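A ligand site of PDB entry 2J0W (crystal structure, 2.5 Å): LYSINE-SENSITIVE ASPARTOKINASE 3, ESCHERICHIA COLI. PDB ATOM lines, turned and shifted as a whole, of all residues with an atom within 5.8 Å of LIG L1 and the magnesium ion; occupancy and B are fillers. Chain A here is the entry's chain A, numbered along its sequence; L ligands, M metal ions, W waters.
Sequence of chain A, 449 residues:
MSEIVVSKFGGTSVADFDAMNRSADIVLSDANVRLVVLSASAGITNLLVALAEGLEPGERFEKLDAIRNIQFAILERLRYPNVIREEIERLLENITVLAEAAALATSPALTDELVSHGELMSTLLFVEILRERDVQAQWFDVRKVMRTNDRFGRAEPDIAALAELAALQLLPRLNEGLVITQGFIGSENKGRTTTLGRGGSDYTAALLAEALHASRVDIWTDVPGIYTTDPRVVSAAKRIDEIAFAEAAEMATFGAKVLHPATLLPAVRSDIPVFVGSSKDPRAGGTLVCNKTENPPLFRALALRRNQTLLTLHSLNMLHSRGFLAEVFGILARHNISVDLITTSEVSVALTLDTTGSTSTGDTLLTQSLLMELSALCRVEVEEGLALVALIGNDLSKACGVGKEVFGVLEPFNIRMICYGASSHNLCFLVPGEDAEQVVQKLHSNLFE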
ATOM      1  N   LYS A   8      19.355 -38.028   3.948  1.00  0.00           N
ATOM      2  CA  LYS A   8      20.130 -37.516   5.064  1.00  0.00           C
ATOM      3  C   LYS A   8      19.850 -36.051   5.352  1.00  0.00           C
ATOM      4  O   LYS A   8      19.795 -35.223   4.446  1.00  0.00           O
ATOM      5  CB  LYS A   8      21.632 -37.728   4.818  1.00  0.00           C
ATOM      6  CG  LYS A   8      22.539 -37.294   5.961  1.00  0.00           C
ATOM      7  CD  LYS A   8      22.903 -35.817   5.900  1.00  0.00           C
ATOM      8  CE  LYS A   8      24.022 -35.497   6.886  1.00  0.00           C
ATOM      9  NZ  LYS A   8      24.618 -34.141   6.729  1.00  0.00           N
ATOM     10  N   PHE A   9      19.675 -35.750   6.640  1.00  0.00           N
ATOM     11  CA  PHE A   9      19.390 -34.393   7.073  1.00  0.00           C
ATOM     12  C   PHE A   9      20.407 -33.912   8.081  1.00  0.00           C
ATOM     13  O   PHE A   9      20.702 -34.600   9.073  1.00  0.00           O
ATOM     14  CB  PHE A   9      17.987 -34.344   7.668  1.00  0.00           C
ATOM     15  CG  PHE A   9      16.911 -34.726   6.698  1.00  0.00           C
ATOM     16  CD1 PHE A   9      16.355 -33.781   5.844  1.00  0.00           C
ATOM     17  CD2 PHE A   9      16.451 -36.051   6.637  1.00  0.00           C
ATOM     18  CE1 PHE A   9      15.351 -34.127   4.942  1.00  0.00           C
ATOM     19  CE2 PHE A   9      15.452 -36.414   5.744  1.00  0.00           C
ATOM     20  CZ  PHE A   9      14.903 -35.446   4.886  1.00  0.00           C
ATOM     21  N   GLY A  10      20.949 -32.727   7.817  1.00  0.00           N
ATOM     22  CA  GLY A  10      21.960 -32.144   8.674  1.00  0.00           C
ATOM     23  C   GLY A  10      21.427 -31.266   9.796  1.00  0.00           C
ATOM     24  O   GLY A  10      20.217 -31.165   9.996  1.00  0.00           O
ATOM     25  N   GLY A  11      22.352 -30.626  10.505  1.00  0.00           N
ATOM     26  CA  GLY A  11      22.001 -29.769  11.627  1.00  0.00           C
ATOM     27  C   GLY A  11      20.851 -28.817  11.340  1.00  0.00           C
ATOM     28  O   GLY A  11      19.775 -28.965  11.910  1.00  0.00           O
ATOM     29  N   THR A  12      21.102 -27.850  10.466  1.00  0.00           N
ATOM     30  CA  THR A  12      20.075 -26.867  10.112  1.00  0.00           C
ATOM     31  C   THR A  12      18.743 -27.514   9.731  1.00  0.00           C
ATOM     32  O   THR A  12      17.681 -26.995  10.071  1.00  0.00           O
ATOM     33  CB  THR A  12      20.531 -26.003   8.941  1.00  0.00           C
ATOM     34  OG1 THR A  12      20.837 -26.837   7.817  1.00  0.00           O
ATOM     35  CG2 THR A  12      21.743 -25.188   9.320  1.00  0.00           C
ATOM     36  N   SER A  13      18.797 -28.657   9.039  1.00  0.00           N
ATOM     37  CA  SER A  13      17.582 -29.332   8.594  1.00  0.00           C
ATOM     38  C   SER A  13      16.747 -29.971   9.700  1.00  0.00           C
ATOM     39  O   SER A  13      15.671 -30.496   9.449  1.00  0.00           O
ATOM     40  CB  SER A  13      17.924 -30.396   7.549  1.00  0.00           C
ATOM     41  OG  SER A  13      18.570 -29.787   6.442  1.00  0.00           O
ATOM     42  N   SER A  39      21.408 -36.001  11.679  1.00  0.00           N
ATOM     43  CA  SER A  39      22.564 -35.532  12.435  1.00  0.00           C
ATOM     44  C   SER A  39      21.823 -34.933  13.625  1.00  0.00           C
ATOM     45  O   SER A  39      20.600 -34.919  13.641  1.00  0.00           O
ATOM     46  CB  SER A  39      23.294 -34.395  11.708  1.00  0.00           C
ATOM     47  OG  SER A  39      23.944 -34.805  10.517  1.00  0.00           O
ATOM     48  N   GLY A 199      31.043 -34.233  10.469  1.00  0.00           N
ATOM     49  CA  GLY A 199      30.414 -34.337   9.168  1.00  0.00           C
ATOM     50  C   GLY A 199      30.149 -35.771   8.743  1.00  0.00           C
ATOM     51  O   GLY A 199      29.683 -36.024   7.640  1.00  0.00           O
ATOM     52  N   GLY A 200      30.435 -36.686   9.653  1.00  0.00           N
ATOM     53  CA  GLY A 200      30.262 -38.099   9.385  1.00  0.00           C
ATOM     54  C   GLY A 200      28.860 -38.571   9.093  1.00  0.00           C
ATOM     55  O   GLY A 200      28.670 -39.709   8.651  1.00  0.00           O
ATOM     56  N   ASP A 202      27.136 -37.743   6.681  1.00  0.00           N
ATOM     57  CA  ASP A 202      27.048 -37.935   5.236  1.00  0.00           C
ATOM     58  C   ASP A 202      27.559 -39.322   4.931  1.00  0.00           C
ATOM     59  O   ASP A 202      26.955 -40.093   4.169  1.00  0.00           O
ATOM     60  CB  ASP A 202      27.941 -36.952   4.453  1.00  0.00           C
ATOM     61  CG  ASP A 202      27.441 -35.535   4.516  1.00  0.00           C
ATOM     62  OD1 ASP A 202      26.202 -35.324   4.407  1.00  0.00           O
ATOM     63  OD2 ASP A 202      28.299 -34.627   4.651  1.00  0.00           O
ATOM     64  N   ILE A 219      21.159 -36.107   0.027  1.00  0.00           N
ATOM     65  CA  ILE A 219      21.772 -35.275   1.054  1.00  0.00           C
ATOM     66  C   ILE A 219      21.020 -33.944   1.132  1.00  0.00           C
ATOM     67  O   ILE A 219      21.089 -33.121   0.219  1.00  0.00           O
ATOM     68  CB  ILE A 219      23.276 -34.980   0.721  1.00  0.00           C
ATOM     69  CG1 ILE A 219      24.042 -36.293   0.566  1.00  0.00           C
ATOM     70  CG2 ILE A 219      23.905 -34.132   1.831  1.00  0.00           C
ATOM     71  CD1 ILE A 219      23.879 -37.243   1.735  1.00  0.00           C
ATOM     72  N   TRP A 220      20.297 -33.734   2.216  1.00  0.00           N
ATOM     73  CA  TRP A 220      19.545 -32.499   2.394  1.00  0.00           C
ATOM     74  C   TRP A 220      20.300 -31.538   3.309  1.00  0.00           C
ATOM     75  O   TRP A 220      20.443 -31.778   4.493  1.00  0.00           O
ATOM     76  CB  TRP A 220      18.157 -32.803   2.945  1.00  0.00           C
ATOM     77  CG  TRP A 220      17.287 -33.530   1.935  1.00  0.00           C
ATOM     78  CD1 TRP A 220      16.968 -34.864   1.914  1.00  0.00           C
ATOM     79  CD2 TRP A 220      16.706 -32.972   0.751  1.00  0.00           C
ATOM     80  NE1 TRP A 220      16.244 -35.170   0.783  1.00  0.00           N
ATOM     81  CE2 TRP A 220      16.064 -34.022   0.059  1.00  0.00           C
ATOM     82  CE3 TRP A 220      16.677 -31.683   0.200  1.00  0.00           C
ATOM     83  CZ2 TRP A 220      15.397 -33.827  -1.157  1.00  0.00           C
ATOM     84  CZ3 TRP A 220      16.012 -31.483  -1.008  1.00  0.00           C
ATOM     85  CH2 TRP A 220      15.382 -32.548  -1.669  1.00  0.00           C
ATOM     86  N   THR A 221      20.791 -30.434   2.744  1.00  0.00           N
ATOM     87  CA  THR A 221      21.545 -29.478   3.528  1.00  0.00           C
ATOM     88  C   THR A 221      20.904 -28.087   3.572  1.00  0.00           C
ATOM     89  O   THR A 221      19.693 -27.970   3.431  1.00  0.00           O
ATOM     90  CB  THR A 221      22.999 -29.368   2.999  1.00  0.00           C
ATOM     91  OG1 THR A 221      23.704 -28.345   3.715  1.00  0.00           O
ATOM     92  CG2 THR A 221      23.000 -29.046   1.537  1.00  0.00           C
ATOM     93  N   ASP A 222      21.719 -27.048   3.769  1.00  0.00           N
ATOM     94  CA  ASP A 222      21.231 -25.674   3.855  1.00  0.00           C
ATOM     95  C   ASP A 222      21.647 -24.860   2.618  1.00  0.00           C
ATOM     96  O   ASP A 222      21.702 -23.630   2.646  1.00  0.00           O
ATOM     97  CB  ASP A 222      21.779 -25.009   5.120  1.00  0.00           C
ATOM     98  CG  ASP A 222      23.271 -24.749   5.059  1.00  0.00           C
ATOM     99  OD1 ASP A 222      23.913 -25.177   4.090  1.00  0.00           O
ATOM    100  OD2 ASP A 222      23.810 -24.096   5.977  1.00  0.00           O
ATOM    101  N   VAL A 223      21.925 -25.573   1.533  1.00  0.00           N
ATOM    102  CA  VAL A 223      22.337 -24.968   0.262  1.00  0.00           C
ATOM    103  C   VAL A 223      21.851 -25.882  -0.845  1.00  0.00           C
ATOM    104  O   VAL A 223      22.126 -27.078  -0.829  1.00  0.00           O
ATOM    105  CB  VAL A 223      23.855 -24.829   0.186  1.00  0.00           C
ATOM    106  CG1 VAL A 223      24.340 -25.123  -1.218  1.00  0.00           C
ATOM    107  CG2 VAL A 223      24.258 -23.422   0.602  1.00  0.00           C
ATOM    108  N   GLY A 225      22.216 -27.785  -3.607  1.00  0.00           N
ATOM    109  CA  GLY A 225      23.197 -28.426  -4.470  1.00  0.00           C
ATOM    110  C   GLY A 225      24.665 -28.140  -4.185  1.00  0.00           C
ATOM    111  O   GLY A 225      25.013 -27.549  -3.160  1.00  0.00           O
ATOM    112  N   ILE A 226      25.536 -28.571  -5.105  1.00  0.00           N
ATOM    113  CA  ILE A 226      26.975 -28.369  -4.991  1.00  0.00           C
ATOM    114  C   ILE A 226      27.345 -27.190  -5.926  1.00  0.00           C
ATOM    115  O   ILE A 226      27.034 -27.226  -7.116  1.00  0.00           O
ATOM    116  CB  ILE A 226      27.748 -29.656  -5.435  1.00  0.00           C
ATOM    117  CG1 ILE A 226      27.305 -30.848  -4.593  1.00  0.00           C
ATOM    118  CG2 ILE A 226      29.251 -29.453  -5.290  1.00  0.00           C
ATOM    119  CD1 ILE A 226      27.893 -32.180  -5.066  1.00  0.00           C
ATOM    120  N   TYR A 227      28.002 -26.176  -5.387  1.00  0.00           N
ATOM    121  CA  TYR A 227      28.372 -25.012  -6.201  1.00  0.00           C
ATOM    122  C   TYR A 227      29.804 -25.061  -6.707  1.00  0.00           C
ATOM    123  O   TYR A 227      30.546 -25.963  -6.363  1.00  0.00           O
ATOM    124  CB  TYR A 227      28.164 -23.729  -5.398  1.00  0.00           C
ATOM    125  CG  TYR A 227      26.710 -23.368  -5.226  1.00  0.00           C
ATOM    126  CD1 TYR A 227      25.791 -24.325  -4.797  1.00  0.00           C
ATOM    127  CD2 TYR A 227      26.244 -22.094  -5.510  1.00  0.00           C
ATOM    128  CE1 TYR A 227      24.458 -24.021  -4.658  1.00  0.00           C
ATOM    129  CE2 TYR A 227      24.897 -21.774  -5.377  1.00  0.00           C
ATOM    130  CZ  TYR A 227      24.011 -22.745  -4.948  1.00  0.00           C
ATOM    131  OH  TYR A 227      22.678 -22.469  -4.816  1.00  0.00           O
ATOM    132  N   THR A 228      30.172 -24.067  -7.508  1.00  0.00           N
ATOM    133  CA  THR A 228      31.527 -23.997  -8.057  1.00  0.00           C
ATOM    134  C   THR A 228      32.527 -23.567  -6.987  1.00  0.00           C
ATOM    135  O   THR A 228      33.710 -23.360  -7.258  1.00  0.00           O
ATOM    136  CB  THR A 228      31.603 -23.011  -9.225  1.00  0.00           C
ATOM    137  OG1 THR A 228      31.176 -21.714  -8.787  1.00  0.00           O
ATOM    138  CG2 THR A 228      30.728 -23.487 -10.374  1.00  0.00           C
ATOM    139  N   THR A 229      32.034 -23.404  -5.765  1.00  0.00           N
ATOM    140  CA  THR A 229      32.876 -23.037  -4.646  1.00  0.00           C
ATOM    141  C   THR A 229      31.967 -22.631  -3.503  1.00  0.00           C
ATOM    142  O   THR A 229      30.792 -22.316  -3.710  1.00  0.00           O
ATOM    143  CB  THR A 229      33.830 -21.890  -4.988  1.00  0.00           C
ATOM    144  OG1 THR A 229      34.919 -21.867  -4.069  1.00  0.00           O
ATOM    145  CG2 THR A 229      33.115 -20.569  -4.926  1.00  0.00           C
ATOM    146  N   ASP A 230      32.495 -22.646  -2.279  1.00  0.00           N
ATOM    147  CA  ASP A 230      31.715 -22.297  -1.110  1.00  0.00           C
ATOM    148  C   ASP A 230      30.991 -20.960  -1.326  1.00  0.00           C
ATOM    149  O   ASP A 230      31.611 -19.908  -1.487  1.00  0.00           O
ATOM    150  CB  ASP A 230      32.637 -22.189   0.119  1.00  0.00           C
ATOM    151  CG  ASP A 230      31.868 -22.184   1.424  1.00  0.00           C
ATOM    152  OD1 ASP A 230      30.869 -21.450   1.531  1.00  0.00           O
ATOM    153  OD2 ASP A 230      32.277 -22.904   2.368  1.00  0.00           O
ATOM    154  N   PRO A 231      29.641 -21.001  -1.325  1.00  0.00           N
ATOM    155  CA  PRO A 231      28.830 -19.794  -1.518  1.00  0.00           C
ATOM    156  C   PRO A 231      29.124 -18.777  -0.449  1.00  0.00           C
ATOM    157  O   PRO A 231      28.888 -17.584  -0.634  1.00  0.00           O
ATOM    158  CB  PRO A 231      27.396 -20.332  -1.414  1.00  0.00           C
ATOM    159  CG  PRO A 231      27.532 -21.680  -2.007  1.00  0.00           C
ATOM    160  CD  PRO A 231      28.775 -22.188  -1.301  1.00  0.00           C
ATOM    161  N   ARG A 232      29.666 -19.240   0.671  1.00  0.00           N
ATOM    162  CA  ARG A 232      29.967 -18.338   1.764  1.00  0.00           C
ATOM    163  C   ARG A 232      31.236 -17.561   1.514  1.00  0.00           C
ATOM    164  O   ARG A 232      31.575 -16.681   2.304  1.00  0.00           O
ATOM    165  CB  ARG A 232      30.100 -19.103   3.073  1.00  0.00           C
ATOM    166  CG  ARG A 232      28.963 -20.013   3.336  1.00  0.00           C
ATOM    167  CD  ARG A 232      29.005 -20.568   4.743  1.00  0.00           C
ATOM    168  NE  ARG A 232      27.866 -21.456   4.943  1.00  0.00           N
ATOM    169  CZ  ARG A 232      27.464 -21.881   6.131  1.00  0.00           C
ATOM    170  NH1 ARG A 232      28.108 -21.510   7.229  1.00  0.00           N
ATOM    171  NH2 ARG A 232      26.418 -22.690   6.217  1.00  0.00           N
ATOM    172  N   MET A 251      36.575 -32.765  -4.754  1.00  0.00           N
ATOM    173  CA  MET A 251      36.086 -31.484  -4.251  1.00  0.00           C
ATOM    174  C   MET A 251      35.945 -31.592  -2.742  1.00  0.00           C
ATOM    175  O   MET A 251      36.410 -30.724  -1.992  1.00  0.00           O
ATOM    176  CB  MET A 251      34.709 -31.131  -4.831  1.00  0.00           C
ATOM    177  CG  MET A 251      34.735 -30.579  -6.254  1.00  0.00           C
ATOM    178  SD  MET A 251      33.137 -29.885  -6.713  1.00  0.00           S
ATOM    179  CE  MET A 251      33.213 -28.264  -5.830  1.00  0.00           C
ATOM    180  N   GLY A 255      38.207 -29.653   0.448  1.00  0.00           N
ATOM    181  CA  GLY A 255      37.546 -28.543   1.087  1.00  0.00           C
ATOM    182  C   GLY A 255      36.053 -28.366   0.875  1.00  0.00           C
ATOM    183  O   GLY A 255      35.474 -27.495   1.512  1.00  0.00           O
ATOM    184  N   ALA A 256      35.447 -29.163   0.007  1.00  0.00           N
ATOM    185  CA  ALA A 256      34.009 -29.056  -0.248  1.00  0.00           C
ATOM    186  C   ALA A 256      33.200 -29.629   0.918  1.00  0.00           C
ATOM    187  O   ALA A 256      32.575 -30.695   0.809  1.00  0.00           O
ATOM    188  CB  ALA A 256      33.657 -29.765  -1.538  1.00  0.00           C
ATOM    189  N   LYS A 257      33.197 -28.902   2.039  1.00  0.00           N
ATOM    190  CA  LYS A 257      32.507 -29.291   3.260  1.00  0.00           C
ATOM    191  C   LYS A 257      31.119 -29.946   3.059  1.00  0.00           C
ATOM    192  O   LYS A 257      30.766 -30.865   3.796  1.00  0.00           O
ATOM    193  CB  LYS A 257      32.381 -28.056   4.170  1.00  0.00           C
ATOM    194  CG  LYS A 257      31.793 -28.279   5.548  1.00  0.00           C
ATOM    195  CD  LYS A 257      31.807 -26.961   6.327  1.00  0.00           C
ATOM    196  CE  LYS A 257      31.565 -27.148   7.830  1.00  0.00           C
ATOM    197  NZ  LYS A 257      30.187 -27.607   8.149  1.00  0.00           N
ATOM    198  N   VAL A 258      30.348 -29.479   2.075  1.00  0.00           N
ATOM    199  CA  VAL A 258      29.028 -30.061   1.844  1.00  0.00           C
ATOM    200  C   VAL A 258      29.073 -31.575   1.851  1.00  0.00           C
ATOM    201  O   VAL A 258      28.065 -32.218   2.125  1.00  0.00           O
ATOM    202  CB  VAL A 258      28.361 -29.583   0.541  1.00  0.00           C
ATOM    203  CG1 VAL A 258      27.615 -28.319   0.809  1.00  0.00           C
ATOM    204  CG2 VAL A 258      29.371 -29.394  -0.565  1.00  0.00           C
ATOM    205  N   ALA A 301      35.213 -26.381 -10.406  1.00  0.00           N
ATOM    206  CA  ALA A 301      35.182 -25.519  -9.243  1.00  0.00           C
ATOM    207  C   ALA A 301      36.501 -25.354  -8.518  1.00  0.00           C
ATOM    208  O   ALA A 301      37.513 -25.895  -8.915  1.00  0.00           O
ATOM    209  CB  ALA A 301      34.141 -26.036  -8.281  1.00  0.00           C
ATOM    210  N   LEU A 302      36.440 -24.595  -7.439  1.00  0.00           N
ATOM    211  CA  LEU A 302      37.583 -24.332  -6.582  1.00  0.00           C
ATOM    212  C   LEU A 302      37.177 -24.783  -5.192  1.00  0.00           C
ATOM    213  O   LEU A 302      36.017 -24.641  -4.799  1.00  0.00           O
ATOM    214  CB  LEU A 302      37.906 -22.835  -6.570  1.00  0.00           C
ATOM    215  CG  LEU A 302      38.213 -22.217  -7.931  1.00  0.00           C
ATOM    216  CD1 LEU A 302      38.327 -20.711  -7.782  1.00  0.00           C
ATOM    217  CD2 LEU A 302      39.500 -22.804  -8.498  1.00  0.00           C
HETATM  218  P1  LIG L   1      25.038 -30.288   6.831  1.00  0.00           P
HETATM  219  O1  LIG L   1      23.831 -30.284   5.976  1.00  0.00           O
HETATM  220  O2  LIG L   1      24.699 -30.303   8.309  1.00  0.00           O
HETATM  221  O3  LIG L   1      25.995 -31.482   6.483  1.00  0.00           O
HETATM  222  P2  LIG L   1      27.291 -28.477   6.524  1.00  0.00           P
HETATM  223  O4  LIG L   1      27.478 -27.146   7.160  1.00  0.00           O
HETATM  224  O5  LIG L   1      28.109 -29.595   7.074  1.00  0.00           O
HETATM  225  O6  LIG L   1      25.774 -28.898   6.563  1.00  0.00           O
HETATM  226  O7  LIG L   1      27.644 -28.141   4.979  1.00  0.00           O
HETATM  227  C1  LIG L   1      26.898 -27.327   4.031  1.00  0.00           C
HETATM  228  C2  LIG L   1      27.771 -26.135   3.682  1.00  0.00           C
HETATM  229  O8  LIG L   1      29.082 -26.414   3.104  1.00  0.00           O
HETATM  230  C3  LIG L   1      27.237 -25.080   2.763  1.00  0.00           C
HETATM  231  O9  LIG L   1      26.207 -24.442   3.543  1.00  0.00           O
HETATM  232  C4  LIG L   1      28.478 -24.258   2.503  1.00  0.00           C
HETATM  233  O10 LIG L   1      28.721 -23.338   3.551  1.00  0.00           O
HETATM  234  C5  LIG L   1      29.576 -25.263   2.434  1.00  0.00           C
HETATM  235  N1  LIG L   1      30.174 -25.513   1.031  1.00  0.00           N
HETATM  236  C6  LIG L   1      31.504 -25.492   0.840  1.00  0.00           C
HETATM  237  N2  LIG L   1      31.901 -25.717  -0.401  1.00  0.00           N
HETATM  238  C7  LIG L   1      30.746 -25.913  -1.053  1.00  0.00           C
HETATM  239  C8  LIG L   1      30.512 -26.189  -2.451  1.00  0.00           C
HETATM  240  N3  LIG L   1      31.436 -26.332  -3.329  1.00  0.00           N
HETATM  241  N4  LIG L   1      29.147 -26.314  -2.796  1.00  0.00           N
HETATM  242  C9  LIG L   1      28.103 -26.177  -1.869  1.00  0.00           C
HETATM  243  N5  LIG L   1      28.333 -25.911  -0.549  1.00  0.00           N
HETATM  244  C10 LIG L   1      29.636 -25.787  -0.198  1.00  0.00           C
HETATM  245  N1  LG2 L   2      26.664 -34.322  14.174  1.00  0.00           N
HETATM  246  C1  LG2 L   2      28.047 -34.414  13.699  1.00  0.00           C
HETATM  247  C2  LG2 L   2      28.592 -32.972  13.634  1.00  0.00           C
HETATM  248  O1  LG2 L   2      27.901 -32.055  14.137  1.00  0.00           O
HETATM  249  C3  LG2 L   2      28.072 -35.161  12.327  1.00  0.00           C
HETATM  250  C4  LG2 L   2      27.428 -34.431  11.123  1.00  0.00           C
HETATM  251  O2  LG2 L   2      26.927 -33.277  11.307  1.00  0.00           O
HETATM  252  O3  LG2 L   2      27.418 -35.012   9.972  1.00  0.00           O
HETATM  253  O4  LG2 L   2      29.709 -32.767  13.040  1.00  0.00           O
HETATM  254 MG    MG M   1      27.836 -32.219   7.245  1.00  0.00          MG
HETATM  255  O   HOH W   1      25.275 -32.971   9.044  1.00  0.00           O
HETATM  256  O   HOH W   2      28.112 -27.626  10.351  1.00  0.00           O
HETATM  257  O   HOH W   3      29.858 -31.472   7.404  1.00  0.00           O
HETATM  258  O   HOH W   4      27.588 -31.128   9.301  1.00  0.00           O
HETATM  259  O   HOH W   5      28.841 -32.401   4.959  1.00  0.00           O
HETATM  260  O   HOH W   6      27.773 -34.112   7.407  1.00  0.00           O
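An oxygen (O1) of LIG L1 sits at hydrogen-bond distance from the side-chain hydroxyl (OG1) of Thr 221 (3.0 Å).
The guanidinium group (NE) of Arg 232 is in hydrogen-bond range of an oxygen (O10) of LIG L1, 2.5 Å away.
The backbone NH (N) of Gly 11 sits at hydrogen-bond distance from an oxygen (O2) of LIG L1.
An oxygen (O4) of LG2 L2 sits at hydrogen-bond distance from the backbone NH (N) of Gly 199, at 3.2 Å.
An oxygen (O3) of LG2 L2 lies within hydrogen-bond range of the backbone NH (N) of Gly 200.
A nitrogen (N4) of LIG L1 is in hydrogen-bond range of the backbone NH (N) of Tyr 227 (2.8 Å).
The side-chain amino group (NZ) of Lys 8 sits close to an oxygen (O3) of LIG L1 (3.0 Å).
The backbone NH of Val 258 lies close to an oxygen (O8) of LIG L1 (3.5 Å).
A nitrogen (N3) of LIG L1 sits at hydrogen-bond distance from the backbone carbonyl oxygen (O) of Tyr 227 (3.2 Å).
The side-chain hydroxyl of Ser 39 sits at hydrogen-bond distance from an oxygen (O2) of LG2 L2, 3.4 Å away.
NZ of Lys 257 lies within salt-bridge range of O4 of LIG L1 (2.9 Å).
The side-chain carboxylate (OD1) of Asp 222 lies within hydrogen-bond range of an oxygen (O9) of LIG L1.
The magnesium ion is bound by water W6, an oxygen (O3) of LIG L1, water W3, water W4 and water W5.
Slightly farther from the magnesium ion lies an oxygen (O5) of LIG L1 (2.6 Å).
Water W6 lies within hydrogen-bond range of the backbone carbonyl oxygen of Gly 199, an oxygen (O3) of LG2 L2, the side-chain carboxylate of Asp 202 and the side-chain amino group of Lys 8.
Water W4 bridges an oxygen (O5) of LIG L1 and an oxygen (O2) of LG2 L2.
Water W1 lies within hydrogen-bond range of NZ of Lys 8 (2.7 Å), OG of Ser 39 (2.7 Å), O2 of LG2 L2 (2.8 Å) and O2 of LIG L1 (2.8 Å).
Water W2 lies within hydrogen-bond range of the side-chain amino group of Lys 257 (3.0 Å) and an oxygen (O4) of LIG L1 (3.3 Å).
Merely in contact with LIG L1: Gly 10 (3.3 Å), Trp 220 (3.99 Å), Val 223 (3.7 Å), Gly 225 (3.6 Å), Ile 226 (3.7 Å), Thr 229 (3.7 Å), Asp 230 (3.1 Å), Pro 231 (3.8 Å), Met 251 (3.6 Å) and Ala 256 (3.95 Å).
Hydrophobic or aromatic side chains that line LIG L1: Val 223, Tyr 227, Pro 231, Met 251 and Val 258.
18 residues have an atom within 4 Å of LIG L1: Lys 8, Gly 10, Gly 11, Trp 220, Thr 221, Asp 222, Val 223, Gly 225, Ile 226, Tyr 227, Thr 229, Asp 230, Pro 231, Arg 232, Met 251, Ala 256, Lys 257 and Val 258.
Lys 8 touches the magnesium ion.
CA of Gly 199 touches the magnesium ion (3.9 Å).
OD2 of Asp 202 touches the magnesium ion, 3.6 Å away.
Of the 30 residues printed, 3 come within 4 Å of the magnesium ion.
OG1 of Thr 229 lies within hydrogen-bond range of O of Leu 302 (3.1 Å).
The backbone carbonyl oxygen (O) of Met 251 lies within hydrogen-bond range of the backbone NH (N) of Ala 256, 2.7 Å away.
N of Arg 232 sits at hydrogen-bond distance from OD1 of Asp 230, at 2.7 Å.
O of Trp 220 sits at hydrogen-bond distance from N of Gly 10.
O of Trp 220 lies within hydrogen-bond range of OG of Ser 13, 3.4 Å away.
The side-chain hydroxyl (OG1) of Thr 221 lies within hydrogen-bond range of the side-chain carboxylate (OD1) of Asp 222, 3.2 Å away.
The backbone carbonyl oxygen (O) of Lys 8 sits at hydrogen-bond distance from the backbone NH (N) of Trp 220.
OD2 of Asp 222 lies within salt-bridge range of NH2 of Arg 232, at 3.0 Å.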
